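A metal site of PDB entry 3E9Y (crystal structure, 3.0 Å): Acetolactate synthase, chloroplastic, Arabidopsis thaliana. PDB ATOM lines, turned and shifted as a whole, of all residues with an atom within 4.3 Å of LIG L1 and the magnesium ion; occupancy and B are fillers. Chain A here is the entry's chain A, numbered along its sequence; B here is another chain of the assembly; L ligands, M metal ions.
The backbone NH of Ser 454 is in hydrogen-bond range of an oxygen (O2) of LIG L1 (2.6 Å).
N2 of LIG L1 sits at hydrogen-bond distance from O of Gly 425, at 2.9 Å.
O5 of LIG L1 lies within hydrogen-bond range of N of Gln 401 (2.8 Å).
The side-chain amide oxygen of Gln 121 of chain B sits at hydrogen-bond distance from an oxygen (O8) of LIG L1, 2.7 Å away.
The backbone NH of Gly 453 is in hydrogen-bond range of an oxygen (O2) of LIG L1, 3.3 Å away.
N of Met 484 sits at hydrogen-bond distance from O5 of LIG L1.
O4 of LIG L1 sits at hydrogen-bond distance from ND1 of His 402 (3.1 Å).
An oxygen (O2) of LIG L1 is in hydrogen-bond range of the side-chain hydroxyl of Ser 454 (2.7 Å).
An oxygen (O4) of LIG L1 sits at hydrogen-bond distance from the backbone NH (N) of His 402 (2.9 Å).
The backbone NH (N) of Gly 483 sits at hydrogen-bond distance from an oxygen (O5) of LIG L1, 3.4 Å away.
A nitrogen (N3) of LIG L1 is in hydrogen-bond range of the backbone NH of Met 427 (3.4 Å).
N4 of LIG L1 sits at hydrogen-bond distance from OE1 of Glu 58 of chain B, 2.6 Å away.
The backbone carbonyl oxygen (O) of Pro 84 of chain B sits close to the side-chain amide oxygen (OD1) of Asn 88 of chain B (3.1 Å).
A ring nitrogen (NE2) of His 402 is in hydrogen-bond range of the backbone NH (N) of Gly 451 (3.2 Å).
The backbone NH (N) of Val 399 sits at hydrogen-bond distance from the side-chain hydroxyl (OG) of Ser 454 (3.4 Å).
The side-chain amide nitrogen of Gln 121 of chain B lies within hydrogen-bond range of the backbone carbonyl oxygen of Gly 425, at 3.3 Å.
OE1 of Gln 401 lies within hydrogen-bond range of ND2 of Asn 479.
Val 399 touches LIG L1 (O to C1, 3.1 Å).
Gly 400 touches LIG L1 (CA to O5, 3.4 Å).
Gly 451 touches LIG L1 (C to O2, 3.5 Å).
CD2 of Leu 482 touches O7 of LIG L1, at 3.4 Å.
CG2 of Val 485 touches C7 of LIG L1 (3.6 Å).
CE2 of Tyr 32 of chain B touches C8 of LIG L1 (3.6 Å).
O of Pro 33 of chain B touches C8 of LIG L1 (3.4 Å).
Gly 34 of chain B touches LIG L1 (CA to C9, 3.3 Å).
Gly 35 of chain B touches LIG L1.
CG2 of Thr 81 of chain B touches C14 of LIG L1, 3.9 Å away.
Pro 84 of chain B touches LIG L1 (CG to N3, 3.6 Å).
Asn 88 of chain B touches LIG L1.
Hydrophobic or aromatic side chains within 4 Å of LIG L1: Val 399, His 402, Met 427, Leu 482, Met 484, Val 485, Tyr 32 of chain B and Pro 84 of chain B.
Of the 29 residues printed, 25 come within 4 Å of LIG L1.
Within 4 Å of the magnesium ion: Asp 452, Asn 479 and His 481.
The magnesium ion is bound by O1 of LIG L1 (2.1 Å), OD1 of Asn 479 (2.3 Å), O6 of LIG L1 (2.3 Å), O of His 481 (2.4 Å) and OD1 of Asp 452 (2.4 Å).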
ATOM      1  N   VAL A 399       9.573  -0.750  -9.757  1.00  0.00           N
ATOM      2  CA  VAL A 399       8.809   0.486  -9.662  1.00  0.00           C
ATOM      3  C   VAL A 399       9.193   1.280  -8.419  1.00  0.00           C
ATOM      4  O   VAL A 399       9.251   0.734  -7.314  1.00  0.00           O
ATOM      5  CB  VAL A 399       7.286   0.208  -9.680  1.00  0.00           C
ATOM      6  CG1 VAL A 399       6.503   1.446  -9.278  1.00  0.00           C
ATOM      7  CG2 VAL A 399       6.875  -0.229 -11.057  1.00  0.00           C
ATOM      8  N   GLY A 400       9.444   2.576  -8.606  1.00  0.00           N
ATOM      9  CA  GLY A 400       9.776   3.460  -7.503  1.00  0.00           C
ATOM     10  C   GLY A 400      10.977   4.331  -7.789  1.00  0.00           C
ATOM     11  O   GLY A 400      11.331   4.557  -8.959  1.00  0.00           O
ATOM     12  N   GLN A 401      11.600   4.822  -6.721  1.00  0.00           N
ATOM     13  CA  GLN A 401      12.737   5.736  -6.831  1.00  0.00           C
ATOM     14  C   GLN A 401      13.764   5.258  -7.849  1.00  0.00           C
ATOM     15  O   GLN A 401      14.182   6.016  -8.711  1.00  0.00           O
ATOM     16  CB  GLN A 401      13.413   5.914  -5.483  1.00  0.00           C
ATOM     17  CG  GLN A 401      12.602   6.667  -4.450  1.00  0.00           C
ATOM     18  CD  GLN A 401      13.385   6.943  -3.185  1.00  0.00           C
ATOM     19  OE1 GLN A 401      14.132   6.077  -2.705  1.00  0.00           O
ATOM     20  NE2 GLN A 401      13.238   8.141  -2.641  1.00  0.00           N
ATOM     21  N   HIS A 402      14.156   3.989  -7.751  1.00  0.00           N
ATOM     22  CA  HIS A 402      15.198   3.452  -8.607  1.00  0.00           C
ATOM     23  C   HIS A 402      14.780   3.485 -10.087  1.00  0.00           C
ATOM     24  O   HIS A 402      15.624   3.635 -10.965  1.00  0.00           O
ATOM     25  CB  HIS A 402      15.591   2.036  -8.174  1.00  0.00           C
ATOM     26  CG  HIS A 402      14.584   0.990  -8.523  1.00  0.00           C
ATOM     27  ND1 HIS A 402      13.420   0.808  -7.807  1.00  0.00           N
ATOM     28  CD2 HIS A 402      14.562   0.067  -9.519  1.00  0.00           C
ATOM     29  CE1 HIS A 402      12.717  -0.182  -8.348  1.00  0.00           C
ATOM     30  NE2 HIS A 402      13.395  -0.643  -9.378  1.00  0.00           N
ATOM     31  N   GLY A 425       2.356   0.401 -13.195  1.00  0.00           N
ATOM     32  CA  GLY A 425       3.441   0.562 -12.226  1.00  0.00           C
ATOM     33  C   GLY A 425       3.553  -0.617 -11.272  1.00  0.00           C
ATOM     34  O   GLY A 425       3.537  -0.438 -10.051  1.00  0.00           O
ATOM     35  N   MET A 427       5.233  -3.590  -9.273  1.00  0.00           N
ATOM     36  CA  MET A 427       6.483  -4.074  -8.686  1.00  0.00           C
ATOM     37  C   MET A 427       6.735  -5.540  -9.060  1.00  0.00           C
ATOM     38  O   MET A 427       5.800  -6.280  -9.381  1.00  0.00           O
ATOM     39  CB  MET A 427       6.467  -3.900  -7.174  1.00  0.00           C
ATOM     40  CG  MET A 427       6.691  -2.485  -6.699  1.00  0.00           C
ATOM     41  SD  MET A 427       6.407  -2.332  -4.932  1.00  0.00           S
ATOM     42  CE  MET A 427       7.795  -3.217  -4.252  1.00  0.00           C
ATOM     43  N   GLY A 451      14.932  -2.552  -7.377  1.00  0.00           N
ATOM     44  CA  GLY A 451      14.947  -2.126  -5.971  1.00  0.00           C
ATOM     45  C   GLY A 451      14.687  -3.320  -5.075  1.00  0.00           C
ATOM     46  O   GLY A 451      14.084  -4.292  -5.508  1.00  0.00           O
ATOM     47  N   ASP A 452      15.138  -3.259  -3.825  1.00  0.00           N
ATOM     48  CA  ASP A 452      15.039  -4.415  -2.923  1.00  0.00           C
ATOM     49  C   ASP A 452      13.592  -4.807  -2.635  1.00  0.00           C
ATOM     50  O   ASP A 452      13.282  -5.986  -2.436  1.00  0.00           O
ATOM     51  CB  ASP A 452      15.852  -4.231  -1.637  1.00  0.00           C
ATOM     52  CG  ASP A 452      15.339  -3.092  -0.774  1.00  0.00           C
ATOM     53  OD1 ASP A 452      15.136  -1.976  -1.296  1.00  0.00           O
ATOM     54  OD2 ASP A 452      15.150  -3.320   0.443  1.00  0.00           O
ATOM     55  N   GLY A 453      12.708  -3.811  -2.606  1.00  0.00           N
ATOM     56  CA  GLY A 453      11.274  -4.077  -2.475  1.00  0.00           C
ATOM     57  C   GLY A 453      10.728  -4.862  -3.654  1.00  0.00           C
ATOM     58  O   GLY A 453      10.057  -5.880  -3.473  1.00  0.00           O
ATOM     59  N   SER A 454      11.019  -4.376  -4.854  1.00  0.00           N
ATOM     60  CA  SER A 454      10.543  -4.988  -6.091  1.00  0.00           C
ATOM     61  C   SER A 454      11.228  -6.316  -6.370  1.00  0.00           C
ATOM     62  O   SER A 454      10.576  -7.278  -6.767  1.00  0.00           O
ATOM     63  CB  SER A 454      10.728  -4.045  -7.272  1.00  0.00           C
ATOM     64  OG  SER A 454      10.064  -2.815  -7.047  1.00  0.00           O
ATOM     65  N   MET A 457       9.915  -9.540  -4.615  1.00  0.00           N
ATOM     66  CA  MET A 457       8.577  -9.979  -5.051  1.00  0.00           C
ATOM     67  C   MET A 457       8.613 -11.125  -6.045  1.00  0.00           C
ATOM     68  O   MET A 457       7.768 -12.028  -5.984  1.00  0.00           O
ATOM     69  CB  MET A 457       7.801  -8.819  -5.682  1.00  0.00           C
ATOM     70  CG  MET A 457       7.432  -7.724  -4.733  1.00  0.00           C
ATOM     71  SD  MET A 457       5.962  -6.912  -5.350  1.00  0.00           S
ATOM     72  CE  MET A 457       5.442  -5.970  -3.917  1.00  0.00           C
ATOM     73  N   ASN A 479      18.200   0.081  -0.800  1.00  0.00           N
ATOM     74  CA  ASN A 479      18.083   1.145   0.202  1.00  0.00           C
ATOM     75  C   ASN A 479      17.201   0.798   1.406  1.00  0.00           C
ATOM     76  O   ASN A 479      16.755   1.689   2.141  1.00  0.00           O
ATOM     77  CB  ASN A 479      17.660   2.480  -0.438  1.00  0.00           C
ATOM     78  CG  ASN A 479      16.208   2.474  -0.921  1.00  0.00           C
ATOM     79  OD1 ASN A 479      15.457   1.513  -0.716  1.00  0.00           O
ATOM     80  ND2 ASN A 479      15.807   3.566  -1.559  1.00  0.00           N
ATOM     81  N   HIS A 481      14.261   0.174   1.991  1.00  0.00           N
ATOM     82  CA  HIS A 481      12.945   0.803   2.113  1.00  0.00           C
ATOM     83  C   HIS A 481      12.132   0.719   0.838  1.00  0.00           C
ATOM     84  O   HIS A 481      12.678   0.543  -0.257  1.00  0.00           O
ATOM     85  CB  HIS A 481      13.092   2.280   2.481  1.00  0.00           C
ATOM     86  CG  HIS A 481      13.486   2.519   3.899  1.00  0.00           C
ATOM     87  ND1 HIS A 481      14.797   2.509   4.324  1.00  0.00           N
ATOM     88  CD2 HIS A 481      12.739   2.789   4.998  1.00  0.00           C
ATOM     89  CE1 HIS A 481      14.848   2.753   5.617  1.00  0.00           C
ATOM     90  NE2 HIS A 481      13.613   2.931   6.050  1.00  0.00           N
ATOM     91  N   LEU A 482      10.814   0.836   0.992  1.00  0.00           N
ATOM     92  CA  LEU A 482       9.927   1.165  -0.125  1.00  0.00           C
ATOM     93  C   LEU A 482      10.073   2.670  -0.373  1.00  0.00           C
ATOM     94  O   LEU A 482       9.270   3.478   0.110  1.00  0.00           O
ATOM     95  CB  LEU A 482       8.475   0.799   0.198  1.00  0.00           C
ATOM     96  CG  LEU A 482       8.170  -0.670   0.496  1.00  0.00           C
ATOM     97  CD1 LEU A 482       6.743  -0.829   0.957  1.00  0.00           C
ATOM     98  CD2 LEU A 482       8.454  -1.530  -0.719  1.00  0.00           C
ATOM     99  N   GLY A 483      11.115   3.027  -1.116  1.00  0.00           N
ATOM    100  CA  GLY A 483      11.581   4.410  -1.257  1.00  0.00           C
ATOM    101  C   GLY A 483      10.574   5.428  -1.751  1.00  0.00           C
ATOM    102  O   GLY A 483      10.465   6.508  -1.177  1.00  0.00           O
ATOM    103  N   MET A 484       9.848   5.082  -2.818  1.00  0.00           N
ATOM    104  CA  MET A 484       8.877   5.996  -3.403  1.00  0.00           C
ATOM    105  C   MET A 484       7.797   6.384  -2.405  1.00  0.00           C
ATOM    106  O   MET A 484       7.382   7.549  -2.343  1.00  0.00           O
ATOM    107  CB  MET A 484       8.267   5.396  -4.669  1.00  0.00           C
ATOM    108  CG  MET A 484       7.440   6.375  -5.498  1.00  0.00           C
ATOM    109  SD  MET A 484       8.376   7.843  -5.995  1.00  0.00           S
ATOM    110  CE  MET A 484       9.226   7.219  -7.439  1.00  0.00           C
ATOM    111  N   VAL A 485       7.337   5.403  -1.621  1.00  0.00           N
ATOM    112  CA  VAL A 485       6.332   5.633  -0.587  1.00  0.00           C
ATOM    113  C   VAL A 485       6.942   6.455   0.540  1.00  0.00           C
ATOM    114  O   VAL A 485       6.290   7.356   1.089  1.00  0.00           O
ATOM    115  CB  VAL A 485       5.759   4.308  -0.041  1.00  0.00           C
ATOM    116  CG1 VAL A 485       4.519   4.559   0.799  1.00  0.00           C
ATOM    117  CG2 VAL A 485       5.420   3.357  -1.191  1.00  0.00           C
ATOM    118  N   LEU A 502      12.002  -2.129   5.049  1.00  0.00           N
ATOM    119  CA  LEU A 502      12.051  -3.508   4.567  1.00  0.00           C
ATOM    120  C   LEU A 502      13.040  -4.415   5.317  1.00  0.00           C
ATOM    121  O   LEU A 502      13.022  -5.632   5.129  1.00  0.00           O
ATOM    122  CB  LEU A 502      12.328  -3.551   3.063  1.00  0.00           C
ATOM    123  CG  LEU A 502      11.250  -3.015   2.113  1.00  0.00           C
ATOM    124  CD1 LEU A 502      11.830  -2.866   0.726  1.00  0.00           C
ATOM    125  CD2 LEU A 502      10.018  -3.912   2.075  1.00  0.00           C
ATOM    126  N   TYR B  32       0.014  -4.117   2.573  1.00  0.00           N
ATOM    127  CA  TYR B  32       1.187  -3.653   1.838  1.00  0.00           C
ATOM    128  C   TYR B  32       0.893  -2.263   1.265  1.00  0.00           C
ATOM    129  O   TYR B  32      -0.093  -2.086   0.555  1.00  0.00           O
ATOM    130  CB  TYR B  32       1.513  -4.634   0.711  1.00  0.00           C
ATOM    131  CG  TYR B  32       2.920  -4.520   0.185  1.00  0.00           C
ATOM    132  CD1 TYR B  32       3.925  -5.357   0.654  1.00  0.00           C
ATOM    133  CD2 TYR B  32       3.244  -3.588  -0.783  1.00  0.00           C
ATOM    134  CE1 TYR B  32       5.226  -5.252   0.170  1.00  0.00           C
ATOM    135  CE2 TYR B  32       4.537  -3.474  -1.280  1.00  0.00           C
ATOM    136  CZ  TYR B  32       5.520  -4.310  -0.805  1.00  0.00           C
ATOM    137  OH  TYR B  32       6.788  -4.181  -1.300  1.00  0.00           O
ATOM    138  N   PRO B  33       1.757  -1.282   1.579  1.00  0.00           N
ATOM    139  CA  PRO B  33       1.440   0.110   1.269  1.00  0.00           C
ATOM    140  C   PRO B  33       1.748   0.517  -0.178  1.00  0.00           C
ATOM    141  O   PRO B  33       2.590  -0.094  -0.848  1.00  0.00           O
ATOM    142  CB  PRO B  33       2.335   0.888   2.236  1.00  0.00           C
ATOM    143  CG  PRO B  33       3.505   0.015   2.442  1.00  0.00           C
ATOM    144  CD  PRO B  33       3.068  -1.409   2.244  1.00  0.00           C
ATOM    145  N   GLY B  34       1.043   1.552  -0.624  1.00  0.00           N
ATOM    146  CA  GLY B  34       1.231   2.135  -1.938  1.00  0.00           C
ATOM    147  C   GLY B  34       0.553   3.489  -2.033  1.00  0.00           C
ATOM    148  O   GLY B  34      -0.127   3.920  -1.092  1.00  0.00           O
ATOM    149  N   GLY B  35       0.718   4.148  -3.166  1.00  0.00           N
ATOM    150  CA  GLY B  35       0.197   5.492  -3.393  1.00  0.00           C
ATOM    151  C   GLY B  35      -1.240   5.722  -2.961  1.00  0.00           C
ATOM    152  O   GLY B  35      -1.530   6.664  -2.223  1.00  0.00           O
ATOM    153  N   GLU B  58       1.749  -9.024  -2.111  1.00  0.00           N
ATOM    154  CA  GLU B  58       0.370  -8.983  -1.622  1.00  0.00           C
ATOM    155  C   GLU B  58      -0.429 -10.277  -1.788  1.00  0.00           C
ATOM    156  O   GLU B  58      -1.457 -10.457  -1.122  1.00  0.00           O
ATOM    157  CB  GLU B  58      -0.372  -7.771  -2.208  1.00  0.00           C
ATOM    158  CG  GLU B  58       0.368  -7.134  -3.359  1.00  0.00           C
ATOM    159  CD  GLU B  58       0.562  -5.650  -3.161  1.00  0.00           C
ATOM    160  OE1 GLU B  58       1.538  -5.110  -3.735  1.00  0.00           O
ATOM    161  OE2 GLU B  58      -0.236  -5.009  -2.451  1.00  0.00           O
ATOM    162  N   THR B  81      -2.896  -1.363  -2.136  1.00  0.00           N
ATOM    163  CA  THR B  81      -3.045  -0.152  -2.930  1.00  0.00           C
ATOM    164  C   THR B  81      -3.852  -0.426  -4.211  1.00  0.00           C
ATOM    165  O   THR B  81      -4.277  -1.558  -4.469  1.00  0.00           O
ATOM    166  CB  THR B  81      -1.671   0.483  -3.260  1.00  0.00           C
ATOM    167  OG1 THR B  81      -1.875   1.818  -3.769  1.00  0.00           O
ATOM    168  CG2 THR B  81      -0.884  -0.333  -4.290  1.00  0.00           C
ATOM    169  N   PRO B  84      -1.716  -2.443  -9.349  1.00  0.00           N
ATOM    170  CA  PRO B  84      -0.966  -3.679  -9.195  1.00  0.00           C
ATOM    171  C   PRO B  84      -1.129  -4.291  -7.807  1.00  0.00           C
ATOM    172  O   PRO B  84      -1.118  -5.523  -7.673  1.00  0.00           O
ATOM    173  CB  PRO B  84       0.489  -3.238  -9.439  1.00  0.00           C
ATOM    174  CG  PRO B  84       0.494  -1.781  -9.115  1.00  0.00           C
ATOM    175  CD  PRO B  84      -0.847  -1.276  -9.542  1.00  0.00           C
ATOM    176  N   GLY B  85      -1.283  -3.456  -6.788  1.00  0.00           N
ATOM    177  CA  GLY B  85      -1.565  -3.926  -5.436  1.00  0.00           C
ATOM    178  C   GLY B  85      -2.839  -4.741  -5.440  1.00  0.00           C
ATOM    179  O   GLY B  85      -2.857  -5.888  -5.000  1.00  0.00           O
ATOM    180  N   ASN B  88      -2.943  -8.145  -7.458  1.00  0.00           N
ATOM    181  CA  ASN B  88      -2.168  -9.207  -6.815  1.00  0.00           C
ATOM    182  C   ASN B  88      -2.941  -9.970  -5.744  1.00  0.00           C
ATOM    183  O   ASN B  88      -2.489 -11.009  -5.265  1.00  0.00           O
ATOM    184  CB  ASN B  88      -0.853  -8.664  -6.257  1.00  0.00           C
ATOM    185  CG  ASN B  88       0.186  -8.427  -7.325  1.00  0.00           C
ATOM    186  OD1 ASN B  88       1.103  -7.615  -7.148  1.00  0.00           O
ATOM    187  ND2 ASN B  88       0.077  -9.140  -8.448  1.00  0.00           N
ATOM    188  N   PHE B 120      -3.116   6.870 -13.309  1.00  0.00           N
ATOM    189  CA  PHE B 120      -1.946   6.225 -12.733  1.00  0.00           C
ATOM    190  C   PHE B 120      -2.357   5.155 -11.727  1.00  0.00           C
ATOM    191  O   PHE B 120      -3.028   5.451 -10.726  1.00  0.00           O
ATOM    192  CB  PHE B 120      -1.049   7.274 -12.069  1.00  0.00           C
ATOM    193  CG  PHE B 120       0.194   6.709 -11.430  1.00  0.00           C
ATOM    194  CD1 PHE B 120       1.176   6.115 -12.204  1.00  0.00           C
ATOM    195  CD2 PHE B 120       0.370   6.795 -10.060  1.00  0.00           C
ATOM    196  CE1 PHE B 120       2.323   5.591 -11.619  1.00  0.00           C
ATOM    197  CE2 PHE B 120       1.514   6.285  -9.458  1.00  0.00           C
ATOM    198  CZ  PHE B 120       2.501   5.681 -10.241  1.00  0.00           C
ATOM    199  N   GLN B 121      -1.958   3.915 -12.016  1.00  0.00           N
ATOM    200  CA  GLN B 121      -2.268   2.745 -11.184  1.00  0.00           C
ATOM    201  C   GLN B 121      -3.773   2.511 -11.020  1.00  0.00           C
ATOM    202  O   GLN B 121      -4.238   2.204  -9.923  1.00  0.00           O
ATOM    203  CB  GLN B 121      -1.582   2.836  -9.822  1.00  0.00           C
ATOM    204  CG  GLN B 121      -0.087   3.037  -9.885  1.00  0.00           C
ATOM    205  CD  GLN B 121       0.616   2.702  -8.584  1.00  0.00           C
ATOM    206  OE1 GLN B 121       0.291   3.253  -7.535  1.00  0.00           O
ATOM    207  NE2 GLN B 121       1.592   1.794  -8.664  1.00  0.00           N
HETATM  208  O1  LIG L   1      12.620  -0.842  -2.949  1.00  0.00           O
HETATM  209  P1  LIG L   1      11.613  -0.570  -4.009  1.00  0.00           P
HETATM  210  O2  LIG L   1      11.490  -1.815  -4.981  1.00  0.00           O
HETATM  211  O3  LIG L   1      12.020   0.670  -4.977  1.00  0.00           O
HETATM  212  P2  LIG L   1      12.586   2.070  -4.454  1.00  0.00           P
HETATM  213  O4  LIG L   1      13.739   2.550  -5.259  1.00  0.00           O
HETATM  214  O5  LIG L   1      11.362   3.125  -4.484  1.00  0.00           O
HETATM  215  O6  LIG L   1      12.967   1.941  -2.893  1.00  0.00           O
HETATM  216  O7  LIG L   1      10.125  -0.303  -3.460  1.00  0.00           O
HETATM  217  C1  LIG L   1       9.076   0.205  -4.291  1.00  0.00           C
HETATM  218  C2  LIG L   1       8.211   1.135  -3.449  1.00  0.00           C
HETATM  219  C3  LIG L   1       6.826   1.386  -4.042  1.00  0.00           C
HETATM  220  S1  LIG L   1       6.603   2.571  -5.274  1.00  0.00           S
HETATM  221  C4  LIG L   1       4.908   2.355  -5.433  1.00  0.00           C
HETATM  222  C5  LIG L   1       4.117   3.035  -6.274  1.00  0.00           C
HETATM  223  C6  LIG L   1       4.692   4.116  -7.193  1.00  0.00           C
HETATM  224  O8  LIG L   1       2.616   2.741  -6.338  1.00  0.00           O
HETATM  225  N1  LIG L   1       4.529   1.241  -4.429  1.00  0.00           N
HETATM  226  C7  LIG L   1       5.595   0.781  -3.731  1.00  0.00           C
HETATM  227  C8  LIG L   1       5.482  -0.320  -2.676  1.00  0.00           C
HETATM  228  C9  LIG L   1       3.149   0.724  -4.281  1.00  0.00           C
HETATM  229  C10 LIG L   1       3.071  -0.642  -5.003  1.00  0.00           C
HETATM  230  C11 LIG L   1       3.353  -0.878  -6.360  1.00  0.00           C
HETATM  231  N2  LIG L   1       3.721   0.107  -7.172  1.00  0.00           N
HETATM  232  N3  LIG L   1       3.259  -2.122  -6.867  1.00  0.00           N
HETATM  233  C12 LIG L   1       2.894  -3.158  -6.091  1.00  0.00           C
HETATM  234  C13 LIG L   1       2.796  -4.556  -6.699  1.00  0.00           C
HETATM  235  N4  LIG L   1       2.620  -2.961  -4.788  1.00  0.00           N
HETATM  236  C14 LIG L   1       2.693  -1.759  -4.242  1.00  0.00           C
HETATM  237  P1  LG2 L   2       1.599   5.181 -23.647  1.00  0.00           P
HETATM  238  O1  LG2 L   2       2.945   4.846 -24.172  1.00  0.00           O
HETATM  239  O2  LG2 L   2       1.050   4.469 -22.459  1.00  0.00           O
HETATM  240  O3  LG2 L   2       0.568   5.008 -24.849  1.00  0.00           O
HETATM  241  C1  LG2 L   2       0.945   5.417 -26.159  1.00  0.00           C
HETATM  242  C2  LG2 L   2      -0.150   6.211 -26.866  1.00  0.00           C
HETATM  243  O4  LG2 L   2       0.266   6.192 -28.244  1.00  0.00           O
HETATM  244  C3  LG2 L   2      -1.521   5.519 -26.800  1.00  0.00           C
HETATM  245  O5  LG2 L   2      -2.542   6.529 -26.718  1.00  0.00           O
HETATM  246  C4  LG2 L   2      -1.613   4.741 -28.107  1.00  0.00           C
HETATM  247  O6  LG2 L   2      -2.971   4.714 -28.567  1.00  0.00           O
HETATM  248  C5  LG2 L   2      -0.775   5.600 -29.060  1.00  0.00           C
HETATM  249  N1  LG2 L   2      -0.068   4.875 -30.151  1.00  0.00           N
HETATM  250  C6  LG2 L   2       0.485   3.668 -30.069  1.00  0.00           C
HETATM  251  N2  LG2 L   2       1.033   3.346 -31.247  1.00  0.00           N
HETATM  252  C7  LG2 L   2       0.832   4.368 -32.073  1.00  0.00           C
HETATM  253  C8  LG2 L   2       1.189   4.581 -33.400  1.00  0.00           C
HETATM  254  N3  LG2 L   2       1.788   3.607 -34.082  1.00  0.00           N
HETATM  255  N4  LG2 L   2       0.937   5.810 -34.028  1.00  0.00           N
HETATM  256  C9  LG2 L   2       0.280   6.942 -33.331  1.00  0.00           C
HETATM  257  N5  LG2 L   2      -0.229   6.543 -31.991  1.00  0.00           N
HETATM  258  C10 LG2 L   2       0.141   5.339 -31.370  1.00  0.00           C
HETATM  259  N6  LG2 L   2       5.729   9.099 -17.050  1.00  0.00           N
HETATM  260  C11 LG2 L   2       6.279  10.324 -17.448  1.00  0.00           C
HETATM  261  O7  LG2 L   2       6.305  10.625 -18.642  1.00  0.00           O
HETATM  262  N7  LG2 L   2       6.797  11.211 -16.493  1.00  0.00           N
HETATM  263  C12 LG2 L   2       6.769  10.861 -15.136  1.00  0.00           C
HETATM  264  O8  LG2 L   2       7.227  11.641 -14.295  1.00  0.00           O
HETATM  265  C13 LG2 L   2       6.209   9.641 -14.737  1.00  0.00           C
HETATM  266  N8  LG2 L   2       6.178   9.287 -13.389  1.00  0.00           N
HETATM  267  C14 LG2 L   2       5.994   7.944 -13.042  1.00  0.00           C
HETATM  268  C15 LG2 L   2       6.330   7.495 -11.767  1.00  0.00           C
HETATM  269  C16 LG2 L   2       6.160   6.158 -11.439  1.00  0.00           C
HETATM  270  C17 LG2 L   2       6.540   5.726 -10.025  1.00  0.00           C
HETATM  271  C18 LG2 L   2       5.638   5.259 -12.375  1.00  0.00           C
HETATM  272  C19 LG2 L   2       5.427   3.774 -12.068  1.00  0.00           C
HETATM  273  C20 LG2 L   2       5.306   5.716 -13.655  1.00  0.00           C
HETATM  274  C21 LG2 L   2       5.467   7.058 -13.982  1.00  0.00           C
HETATM  275  N9  LG2 L   2       5.152   7.524 -15.273  1.00  0.00           N
HETATM  276  C22 LG2 L   2       5.687   8.766 -15.697  1.00  0.00           C
HETATM  277  C23 LG2 L   2       4.383   6.657 -16.196  1.00  0.00           C
HETATM  278  C24 LG2 L   2       3.045   7.249 -16.628  1.00  0.00           C
HETATM  279  O9  LG2 L   2       2.036   6.919 -15.678  1.00  0.00           O
HETATM  280  C25 LG2 L   2       2.633   6.685 -17.981  1.00  0.00           C
HETATM  281  O10 LG2 L   2       3.048   5.322 -18.067  1.00  0.00           O
HETATM  282  C26 LG2 L   2       3.226   7.454 -19.165  1.00  0.00           C
HETATM  283  O11 LG2 L   2       3.236   8.847 -18.895  1.00  0.00           O
HETATM  284  C27 LG2 L   2       2.398   7.219 -20.421  1.00  0.00           C
HETATM  285  O12 LG2 L   2       3.227   7.183 -21.577  1.00  0.00           O
HETATM  286  P2  LG2 L   2       2.656   7.744 -22.985  1.00  0.00           P
HETATM  287  O13 LG2 L   2       2.005   9.056 -22.745  1.00  0.00           O
HETATM  288  O14 LG2 L   2       3.738   7.602 -23.983  1.00  0.00           O
HETATM  289  O15 LG2 L   2       1.449   6.754 -23.347  1.00  0.00           O
HETATM  290  O1  LG3 L   3      -3.242   6.402  -6.819  1.00  0.00           O
HETATM  291  N1  LG3 L   3      -3.242   7.814  -6.647  1.00  0.00           N
HETATM  292  O2  LG3 L   3      -3.025   8.305  -5.342  1.00  0.00           O
HETATM  293  C1  LG3 L   3      -3.454   8.609  -7.711  1.00  0.00           C
HETATM  294  C2  LG3 L   3      -3.667   7.969  -8.923  1.00  0.00           C
HETATM  295  C3  LG3 L   3      -3.895   8.635 -10.118  1.00  0.00           C
HETATM  296  C4  LG3 L   3      -3.941  10.031 -10.247  1.00  0.00           C
HETATM  297  C5  LG3 L   3      -3.726  10.845  -8.966  1.00  0.00           C
HETATM  298  C6  LG3 L   3      -3.471  10.014  -7.703  1.00  0.00           C
HETATM  299  S1  LG3 L   3      -3.234  10.983  -6.247  1.00  0.00           S
HETATM  300  O3  LG3 L   3      -2.936  12.392  -6.642  1.00  0.00           O
HETATM  301  O4  LG3 L   3      -4.497  10.981  -5.454  1.00  0.00           O
HETATM  302  N2  LG3 L   3      -2.001  10.470  -5.258  1.00  0.00           N
HETATM  303  C7  LG3 L   3      -0.817  10.138  -5.808  1.00  0.00           C
HETATM  304  O5  LG3 L   3      -0.520  10.443  -6.960  1.00  0.00           O
HETATM  305  N3  LG3 L   3      -0.017   9.456  -4.982  1.00  0.00           N
HETATM  306  C8  LG3 L   3       1.223   8.999  -5.261  1.00  0.00           C
HETATM  307  N4  LG3 L   3       1.762   9.074  -6.495  1.00  0.00           N
HETATM  308  C9  LG3 L   3       2.976   8.611  -6.763  1.00  0.00           C
HETATM  309  C10 LG3 L   3       3.756   8.010  -5.769  1.00  0.00           C
HETATM  310  C11 LG3 L   3       3.242   7.913  -4.488  1.00  0.00           C
HETATM  311  C12 LG3 L   3       3.982   7.320  -3.473  1.00  0.00           C
HETATM  312  N5  LG3 L   3       1.952   8.404  -4.218  1.00  0.00           N
HETATM  313 MG    MG M   1      14.194   0.141  -2.028  1.00  0.00          MG
